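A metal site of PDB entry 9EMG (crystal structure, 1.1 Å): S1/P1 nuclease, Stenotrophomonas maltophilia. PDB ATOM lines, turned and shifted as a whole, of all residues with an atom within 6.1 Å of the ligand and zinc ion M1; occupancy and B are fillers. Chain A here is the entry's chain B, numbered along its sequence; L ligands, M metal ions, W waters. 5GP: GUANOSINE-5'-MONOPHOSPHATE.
N1 of the ligand is in hydrogen-bond range of OD1 of Asn 65, 2.7 Å away. ND2 of Asn 135 lies within hydrogen-bond range of O4' of the ligand. A nitrogen (N2) of the ligand sits at hydrogen-bond distance from the backbone carbonyl oxygen of Met 124. O3P of the ligand lies within salt-bridge range of NZ of Lys 132 (3.3 Å).
A ring nitrogen (ND1) of His 149 is in hydrogen-bond range of the backbone carbonyl oxygen (O) of Met 124, at 3.5 Å. A ring nitrogen (ND1) of His 149 sits at hydrogen-bond distance from the backbone carbonyl oxygen (O) of Gly 133 (2.8 Å). The backbone NH of His 149 sits at hydrogen-bond distance from the backbone carbonyl oxygen of Gly 134, 3.4 Å away. The backbone NH (N) of Asp 153 lies close to the side-chain amide nitrogen (NE2) of Gln 122 (3.4 Å). The backbone carbonyl oxygen (O) of Asp 153 is in hydrogen-bond range of the backbone NH (N) of Gly 2, at 3.0 Å. O of His 125 sits at hydrogen-bond distance from N of Val 64 (2.9 Å). O of Tyr 128 lies close to OD1 of Asn 65, at 3.5 Å. The backbone NH (N) of Gly 133 sits at hydrogen-bond distance from the backbone carbonyl oxygen (O) of Tyr 128, 2.9 Å away.
CB of His 62 touches O2' of the ligand, at 3.8 Å. Tyr 63 touches the ligand (CE1 to C6, 3.3 Å). CA of Gly 133 touches N2 of the ligand, at 3.4 Å. Hydrophobic or aromatic side chains within 4 Å of the ligand: His 62, Tyr 63, His 125 and His 149. Of the 23 residues printed, 10 come within 4 Å of the ligand. The nearest printed residue that does not touch the ligand is Ala 126 (4.2 Å).
The nearest printed residue that does not touch zinc ion M1 is Trp 1 (4.3 Å).
Zinc ion M1 is bound by NE2 of His 149, water W5, OD2 of Asp 153, NE2 of His 125, O3' of the ligand and OD1 of Asp 153. Zinc ion M1 has six donor atoms within binding distance.
Water W1 bridges an oxygen (O6) of the ligand (2.7 Å) and the backbone carbonyl oxygen (O) of Ala 129 (2.8 Å). Water W4 bridges O of Ala 59 and O2' of the ligand.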
ATOM      1  N   TRP A   1     -14.897  23.013 -11.669  1.00  0.00           N
ATOM      2  CA  TRP A   1     -15.813  24.155 -11.580  1.00  0.00           C
ATOM      3  C   TRP A   1     -15.542  24.959 -10.312  1.00  0.00           C
ATOM      4  O   TRP A   1     -15.009  24.417  -9.338  1.00  0.00           O
ATOM      5  CB  TRP A   1     -17.266  23.684 -11.542  1.00  0.00           C
ATOM      6  CG  TRP A   1     -17.662  22.774 -12.658  1.00  0.00           C
ATOM      7  CD1 TRP A   1     -17.753  21.423 -12.609  1.00  0.00           C
ATOM      8  CD2 TRP A   1     -17.981  23.152 -14.003  1.00  0.00           C
ATOM      9  NE1 TRP A   1     -18.122  20.927 -13.813  1.00  0.00           N
ATOM     10  CE2 TRP A   1     -18.268  21.966 -14.690  1.00  0.00           C
ATOM     11  CE3 TRP A   1     -18.085  24.377 -14.675  1.00  0.00           C
ATOM     12  CZ2 TRP A   1     -18.657  21.949 -16.018  1.00  0.00           C
ATOM     13  CZ3 TRP A   1     -18.444  24.350 -15.999  1.00  0.00           C
ATOM     14  CH2 TRP A   1     -18.742  23.157 -16.662  1.00  0.00           C
ATOM     15  N   GLY A   2     -16.037  26.188 -10.267  1.00  0.00           N
ATOM     16  CA  GLY A   2     -16.193  26.917  -9.002  1.00  0.00           C
ATOM     17  C   GLY A   2     -17.341  26.359  -8.186  1.00  0.00           C
ATOM     18  O   GLY A   2     -18.017  25.360  -8.593  1.00  0.00           O
ATOM     19  N   ASP A  45     -12.611  21.382  -2.765  1.00  0.00           N
ATOM     20  CA  ASP A  45     -11.804  22.560  -3.172  1.00  0.00           C
ATOM     21  C   ASP A  45     -11.438  23.425  -1.963  1.00  0.00           C
ATOM     22  O   ASP A  45     -10.689  24.403  -2.151  1.00  0.00           O
ATOM     23  CB  ASP A  45     -12.538  23.421  -4.192  1.00  0.00           C
ATOM     24  CG  ASP A  45     -12.564  22.906  -5.623  1.00  0.00           C
ATOM     25  OD1 ASP A  45     -11.802  21.982  -5.976  1.00  0.00           O
ATOM     26  OD2 ASP A  45     -13.376  23.493  -6.414  1.00  0.00           O
ATOM     27  N   ARG A  48      -7.557  23.331   1.945  1.00  0.00           N
ATOM     28  CA  ARG A  48      -6.430  24.163   2.472  1.00  0.00           C
ATOM     29  C   ARG A  48      -6.816  24.652   3.880  1.00  0.00           C
ATOM     30  O   ARG A  48      -5.987  24.512   4.807  1.00  0.00           O
ATOM     31  CB  ARG A  48      -6.112  25.344   1.538  1.00  0.00           C
ATOM     32  CG  ARG A  48      -5.325  24.952   0.298  1.00  0.00           C
ATOM     33  CD  ARG A  48      -4.744  26.156  -0.426  1.00  0.00           C
ATOM     34  NE  ARG A  48      -5.772  27.116  -0.800  1.00  0.00           N
ATOM     35  CZ  ARG A  48      -6.579  27.009  -1.856  1.00  0.00           C
ATOM     36  NH1 ARG A  48      -7.474  27.957  -2.099  1.00  0.00           N
ATOM     37  NH2 ARG A  48      -6.494  25.968  -2.674  1.00  0.00           N
ATOM     38  N   ALA A  59      -4.974  17.285  -4.177  1.00  0.00           N
ATOM     39  CA  ALA A  59      -5.053  18.431  -5.120  1.00  0.00           C
ATOM     40  C   ALA A  59      -5.035  17.951  -6.577  1.00  0.00           C
ATOM     41  O   ALA A  59      -5.790  18.509  -7.423  1.00  0.00           O
ATOM     42  CB  ALA A  59      -3.932  19.396  -4.839  1.00  0.00           C
ATOM     43  N   HIS A  62      -8.195  16.474  -9.015  1.00  0.00           N
ATOM     44  CA  HIS A  62      -9.259  17.299  -9.625  1.00  0.00           C
ATOM     45  C   HIS A  62      -9.147  17.337 -11.147  1.00  0.00           C
ATOM     46  O   HIS A  62     -10.063  17.880 -11.790  1.00  0.00           O
ATOM     47  CB  HIS A  62      -9.258  18.714  -9.042  1.00  0.00           C
ATOM     48  CG  HIS A  62      -9.621  18.753  -7.597  1.00  0.00           C
ATOM     49  ND1 HIS A  62     -10.690  19.470  -7.101  1.00  0.00           N
ATOM     50  CD2 HIS A  62      -8.980  18.196  -6.545  1.00  0.00           C
ATOM     51  CE1 HIS A  62     -10.696  19.329  -5.788  1.00  0.00           C
ATOM     52  NE2 HIS A  62      -9.669  18.543  -5.418  1.00  0.00           N
ATOM     53  N   TYR A  63      -8.083  16.831 -11.726  1.00  0.00           N
ATOM     54  CA  TYR A  63      -7.849  17.015 -13.180  1.00  0.00           C
ATOM     55  C   TYR A  63      -7.026  15.848 -13.708  1.00  0.00           C
ATOM     56  O   TYR A  63      -6.514  15.000 -12.958  1.00  0.00           O
ATOM     57  CB  TYR A  63      -7.190  18.362 -13.467  1.00  0.00           C
ATOM     58  CG  TYR A  63      -5.915  18.564 -12.707  1.00  0.00           C
ATOM     59  CD1 TYR A  63      -4.713  18.049 -13.168  1.00  0.00           C
ATOM     60  CD2 TYR A  63      -5.919  19.240 -11.501  1.00  0.00           C
ATOM     61  CE1 TYR A  63      -3.538  18.217 -12.457  1.00  0.00           C
ATOM     62  CE2 TYR A  63      -4.740  19.432 -10.788  1.00  0.00           C
ATOM     63  CZ  TYR A  63      -3.547  18.886 -11.247  1.00  0.00           C
ATOM     64  OH  TYR A  63      -2.373  19.042 -10.563  1.00  0.00           O
ATOM     65  N   VAL A  64      -6.898  15.827 -15.014  1.00  0.00           N
ATOM     66  CA  VAL A  64      -6.010  14.881 -15.728  1.00  0.00           C
ATOM     67  C   VAL A  64      -5.548  15.584 -16.983  1.00  0.00           C
ATOM     68  O   VAL A  64      -6.352  16.245 -17.643  1.00  0.00           O
ATOM     69  CB  VAL A  64      -6.698  13.538 -16.011  1.00  0.00           C
ATOM     70  CG1 VAL A  64      -7.922  13.665 -16.891  1.00  0.00           C
ATOM     71  CG2 VAL A  64      -5.702  12.527 -16.541  1.00  0.00           C
ATOM     72  N   ASN A  65      -4.277  15.465 -17.300  1.00  0.00           N
ATOM     73  CA  ASN A  65      -3.689  16.190 -18.449  1.00  0.00           C
ATOM     74  C   ASN A  65      -3.526  15.197 -19.588  1.00  0.00           C
ATOM     75  O   ASN A  65      -2.482  14.525 -19.661  1.00  0.00           O
ATOM     76  CB  ASN A  65      -2.382  16.873 -18.061  1.00  0.00           C
ATOM     77  CG  ASN A  65      -2.579  17.931 -17.000  1.00  0.00           C
ATOM     78  OD1 ASN A  65      -3.564  18.677 -17.054  1.00  0.00           O
ATOM     79  ND2 ASN A  65      -1.668  18.004 -16.051  1.00  0.00           N
ATOM     80  N   ASP A 119     -16.003  17.837 -11.586  1.00  0.00           N
ATOM     81  CA  ASP A 119     -14.749  18.292 -12.214  1.00  0.00           C
ATOM     82  C   ASP A 119     -14.458  17.503 -13.491  1.00  0.00           C
ATOM     83  O   ASP A 119     -13.902  18.099 -14.426  1.00  0.00           O
ATOM     84  CB  ASP A 119     -13.571  18.182 -11.254  1.00  0.00           C
ATOM     85  CG  ASP A 119     -13.398  19.412 -10.387  1.00  0.00           C
ATOM     86  OD1 ASP A 119     -14.111  20.426 -10.671  1.00  0.00           O
ATOM     87  OD2 ASP A 119     -12.544  19.360  -9.463  1.00  0.00           O
ATOM     88  N   GLN A 122     -15.778  19.170 -16.522  1.00  0.00           N
ATOM     89  CA  GLN A 122     -15.316  20.514 -16.878  1.00  0.00           C
ATOM     90  C   GLN A 122     -14.232  20.313 -17.922  1.00  0.00           C
ATOM     91  O   GLN A 122     -13.160  19.775 -17.586  1.00  0.00           O
ATOM     92  CB  GLN A 122     -14.812  21.219 -15.620  1.00  0.00           C
ATOM     93  CG  GLN A 122     -14.876  22.737 -15.635  1.00  0.00           C
ATOM     94  CD  GLN A 122     -13.941  23.442 -16.579  1.00  0.00           C
ATOM     95  OE1 GLN A 122     -13.921  23.202 -17.775  1.00  0.00           O
ATOM     96  NE2 GLN A 122     -13.159  24.354 -16.043  1.00  0.00           N
ATOM     97  N   MET A 124     -11.792  21.921 -19.194  1.00  0.00           N
ATOM     98  CA  MET A 124     -10.422  22.384 -18.925  1.00  0.00           C
ATOM     99  C   MET A 124      -9.790  21.635 -17.732  1.00  0.00           C
ATOM    100  O   MET A 124      -8.594  21.829 -17.472  1.00  0.00           O
ATOM    101  CB  MET A 124     -10.375  23.895 -18.703  1.00  0.00           C
ATOM    102  CG  MET A 124     -11.028  24.728 -19.831  1.00  0.00           C
ATOM    103  SD  MET A 124     -10.543  24.314 -21.519  1.00  0.00           S
ATOM    104  CE  MET A 124      -8.801  24.736 -21.404  1.00  0.00           C
ATOM    105  N   HIS A 125     -10.532  20.762 -17.081  1.00  0.00           N
ATOM    106  CA  HIS A 125      -9.961  19.810 -16.108  1.00  0.00           C
ATOM    107  C   HIS A 125      -9.419  18.555 -16.810  1.00  0.00           C
ATOM    108  O   HIS A 125      -8.931  17.667 -16.075  1.00  0.00           O
ATOM    109  CB  HIS A 125     -11.003  19.455 -15.051  1.00  0.00           C
ATOM    110  CG  HIS A 125     -11.123  20.512 -14.002  1.00  0.00           C
ATOM    111  ND1 HIS A 125     -10.884  20.251 -12.659  1.00  0.00           N
ATOM    112  CD2 HIS A 125     -11.446  21.829 -14.093  1.00  0.00           C
ATOM    113  CE1 HIS A 125     -10.995  21.370 -11.967  1.00  0.00           C
ATOM    114  NE2 HIS A 125     -11.341  22.359 -12.831  1.00  0.00           N
ATOM    115  N   ALA A 126      -9.458  18.485 -18.136  1.00  0.00           N
ATOM    116  CA  ALA A 126      -8.946  17.326 -18.896  1.00  0.00           C
ATOM    117  C   ALA A 126      -8.114  17.795 -20.090  1.00  0.00           C
ATOM    118  O   ALA A 126      -8.049  17.082 -21.101  1.00  0.00           O
ATOM    119  CB  ALA A 126     -10.089  16.415 -19.285  1.00  0.00           C
ATOM    120  N   GLY A 127      -7.493  18.958 -19.949  1.00  0.00           N
ATOM    121  CA  GLY A 127      -6.738  19.585 -21.042  1.00  0.00           C
ATOM    122  C   GLY A 127      -5.249  19.299 -21.009  1.00  0.00           C
ATOM    123  O   GLY A 127      -4.798  18.177 -20.783  1.00  0.00           O
ATOM    124  N   TYR A 128      -4.467  20.321 -21.354  1.00  0.00           N
ATOM    125  CA  TYR A 128      -3.002  20.196 -21.469  1.00  0.00           C
ATOM    126  C   TYR A 128      -2.318  20.330 -20.098  1.00  0.00           C
ATOM    127  O   TYR A 128      -2.666  21.193 -19.279  1.00  0.00           O
ATOM    128  CB  TYR A 128      -2.413  21.313 -22.320  1.00  0.00           C
ATOM    129  CG  TYR A 128      -2.752  21.332 -23.792  1.00  0.00           C
ATOM    130  CD1 TYR A 128      -2.306  20.342 -24.660  1.00  0.00           C
ATOM    131  CD2 TYR A 128      -3.369  22.444 -24.332  1.00  0.00           C
ATOM    132  CE1 TYR A 128      -2.563  20.398 -26.009  1.00  0.00           C
ATOM    133  CE2 TYR A 128      -3.601  22.530 -25.693  1.00  0.00           C
ATOM    134  CZ  TYR A 128      -3.193  21.513 -26.539  1.00  0.00           C
ATOM    135  OH  TYR A 128      -3.411  21.608 -27.882  1.00  0.00           O
ATOM    136  N   ALA A 129      -1.219  19.591 -19.932  1.00  0.00           N
ATOM    137  CA  ALA A 129      -0.257  19.857 -18.845  1.00  0.00           C
ATOM    138  C   ALA A 129       0.427  21.205 -19.080  1.00  0.00           C
ATOM    139  O   ALA A 129       0.648  21.961 -18.092  1.00  0.00           O
ATOM    140  CB  ALA A 129       0.787  18.766 -18.753  1.00  0.00           C
ATOM    141  N   LYS A 132      -1.440  24.159 -17.938  1.00  0.00           N
ATOM    142  CA  LYS A 132      -2.177  23.939 -16.673  1.00  0.00           C
ATOM    143  C   LYS A 132      -3.697  23.992 -16.937  1.00  0.00           C
ATOM    144  O   LYS A 132      -4.400  24.773 -16.227  1.00  0.00           O
ATOM    145  CB  LYS A 132      -1.698  24.984 -15.656  1.00  0.00           C
ATOM    146  CG  LYS A 132      -2.034  24.711 -14.196  1.00  0.00           C
ATOM    147  CD  LYS A 132      -1.410  25.709 -13.239  1.00  0.00           C
ATOM    148  CE  LYS A 132      -2.105  25.827 -11.893  1.00  0.00           C
ATOM    149  NZ  LYS A 132      -1.305  26.662 -10.951  1.00  0.00           N
ATOM    150  N   GLY A 133      -4.191  23.255 -17.925  1.00  0.00           N
ATOM    151  CA  GLY A 133      -5.639  23.254 -18.179  1.00  0.00           C
ATOM    152  C   GLY A 133      -6.155  24.643 -18.541  1.00  0.00           C
ATOM    153  O   GLY A 133      -7.288  24.989 -18.187  1.00  0.00           O
ATOM    154  N   GLY A 134      -5.340  25.434 -19.215  1.00  0.00           N
ATOM    155  CA  GLY A 134      -5.709  26.786 -19.673  1.00  0.00           C
ATOM    156  C   GLY A 134      -5.437  27.846 -18.635  1.00  0.00           C
ATOM    157  O   GLY A 134      -5.639  29.048 -18.931  1.00  0.00           O
ATOM    158  N   ASN A 135      -4.988  27.477 -17.437  1.00  0.00           N
ATOM    159  CA  ASN A 135      -4.670  28.508 -16.410  1.00  0.00           C
ATOM    160  C   ASN A 135      -3.614  29.473 -16.911  1.00  0.00           C
ATOM    161  O   ASN A 135      -3.637  30.632 -16.506  1.00  0.00           O
ATOM    162  CB  ASN A 135      -4.158  27.933 -15.100  1.00  0.00           C
ATOM    163  CG  ASN A 135      -5.267  27.528 -14.161  1.00  0.00           C
ATOM    164  OD1 ASN A 135      -5.911  28.364 -13.529  1.00  0.00           O
ATOM    165  ND2 ASN A 135      -5.528  26.243 -14.090  1.00  0.00           N
ATOM    166  N   HIS A 149      -8.920  28.752 -17.993  1.00  0.00           N
ATOM    167  CA  HIS A 149      -9.408  27.749 -17.028  1.00  0.00           C
ATOM    168  C   HIS A 149     -10.558  28.344 -16.202  1.00  0.00           C
ATOM    169  O   HIS A 149     -11.636  27.729 -16.074  1.00  0.00           O
ATOM    170  CB  HIS A 149      -8.264  27.245 -16.138  1.00  0.00           C
ATOM    171  CG  HIS A 149      -8.687  26.120 -15.277  1.00  0.00           C
ATOM    172  ND1 HIS A 149      -8.546  24.789 -15.638  1.00  0.00           N
ATOM    173  CD2 HIS A 149      -9.344  26.123 -14.101  1.00  0.00           C
ATOM    174  CE1 HIS A 149      -9.118  24.030 -14.703  1.00  0.00           C
ATOM    175  NE2 HIS A 149      -9.634  24.828 -13.747  1.00  0.00           N
ATOM    176  N   ASP A 153     -14.407  27.420 -15.412  1.00  0.00           N
ATOM    177  CA  ASP A 153     -14.814  27.026 -14.055  1.00  0.00           C
ATOM    178  C   ASP A 153     -15.984  27.869 -13.552  1.00  0.00           C
ATOM    179  O   ASP A 153     -16.880  27.316 -12.883  1.00  0.00           O
ATOM    180  CB  ASP A 153     -13.677  27.207 -13.057  1.00  0.00           C
ATOM    181  CG  ASP A 153     -12.798  25.993 -12.805  1.00  0.00           C
ATOM    182  OD1 ASP A 153     -13.116  24.893 -13.279  1.00  0.00           O
ATOM    183  OD2 ASP A 153     -11.754  26.202 -12.150  1.00  0.00           O
HETATM  184  P   5GP L   1      -4.550  25.935  -8.534  1.00  0.00           P
HETATM  185  O1P 5GP L   1      -3.753  24.746  -8.182  1.00  0.00           O
HETATM  186  O2P 5GP L   1      -5.615  26.280  -7.461  1.00  0.00           O
HETATM  187  O3P 5GP L   1      -3.727  27.194  -8.780  1.00  0.00           O
HETATM  188  O5' 5GP L   1      -5.350  25.596  -9.875  1.00  0.00           O
HETATM  189  C5' 5GP L   1      -6.393  26.429 -10.392  1.00  0.00           C
HETATM  190  C4' 5GP L   1      -7.373  25.517 -11.084  1.00  0.00           C
HETATM  191  O4' 5GP L   1      -6.722  24.787 -12.135  1.00  0.00           O
HETATM  192  C3' 5GP L   1      -8.025  24.471 -10.184  1.00  0.00           C
HETATM  193  O3' 5GP L   1      -9.351  24.331 -10.667  1.00  0.00           O
HETATM  194  C2' 5GP L   1      -7.119  23.244 -10.369  1.00  0.00           C
HETATM  195  O2' 5GP L   1      -7.824  22.014 -10.116  1.00  0.00           O
HETATM  196  C1' 5GP L   1      -6.712  23.398 -11.847  1.00  0.00           C
HETATM  197  N9  5GP L   1      -5.374  22.866 -12.251  1.00  0.00           N
HETATM  198  C8  5GP L   1      -4.181  22.967 -11.600  1.00  0.00           C
HETATM  199  N7  5GP L   1      -3.206  22.311 -12.193  1.00  0.00           N
HETATM  200  C5  5GP L   1      -3.794  21.780 -13.324  1.00  0.00           C
HETATM  201  C6  5GP L   1      -3.256  20.936 -14.349  1.00  0.00           C
HETATM  202  O6  5GP L   1      -2.087  20.544 -14.481  1.00  0.00           O
HETATM  203  N1  5GP L   1      -4.218  20.601 -15.279  1.00  0.00           N
HETATM  204  C2  5GP L   1      -5.535  21.028 -15.254  1.00  0.00           C
HETATM  205  N2  5GP L   1      -6.339  20.558 -16.200  1.00  0.00           N
HETATM  206  N3  5GP L   1      -6.022  21.809 -14.313  1.00  0.00           N
HETATM  207  C4  5GP L   1      -5.121  22.126 -13.385  1.00  0.00           C
HETATM  208 ZN    ZN M   1     -10.854  24.310 -12.191  1.00  0.00          ZN
HETATM  209 ZN    ZN M   2     -14.398  22.277  -9.759  1.00  0.00          ZN
HETATM  210 ZN    ZN M   3     -12.191  20.607  -7.877  1.00  0.00          ZN
HETATM  211  O   HOH W   1       0.280  21.644 -15.294  1.00  0.00           O
HETATM  212  O   HOH W   2      -4.296  22.305  -7.897  1.00  0.00           O
HETATM  213  O   HOH W   3      -9.890  24.320  -7.920  1.00  0.00           O
HETATM  214  O   HOH W   4      -6.743  21.024  -7.614  1.00  0.00           O
HETATM  215  O   HOH W   5     -11.853  24.105 -10.388  1.00  0.00           O
HETATM  216  O   HOH W   6     -10.054  21.954  -8.673  1.00  0.00           O
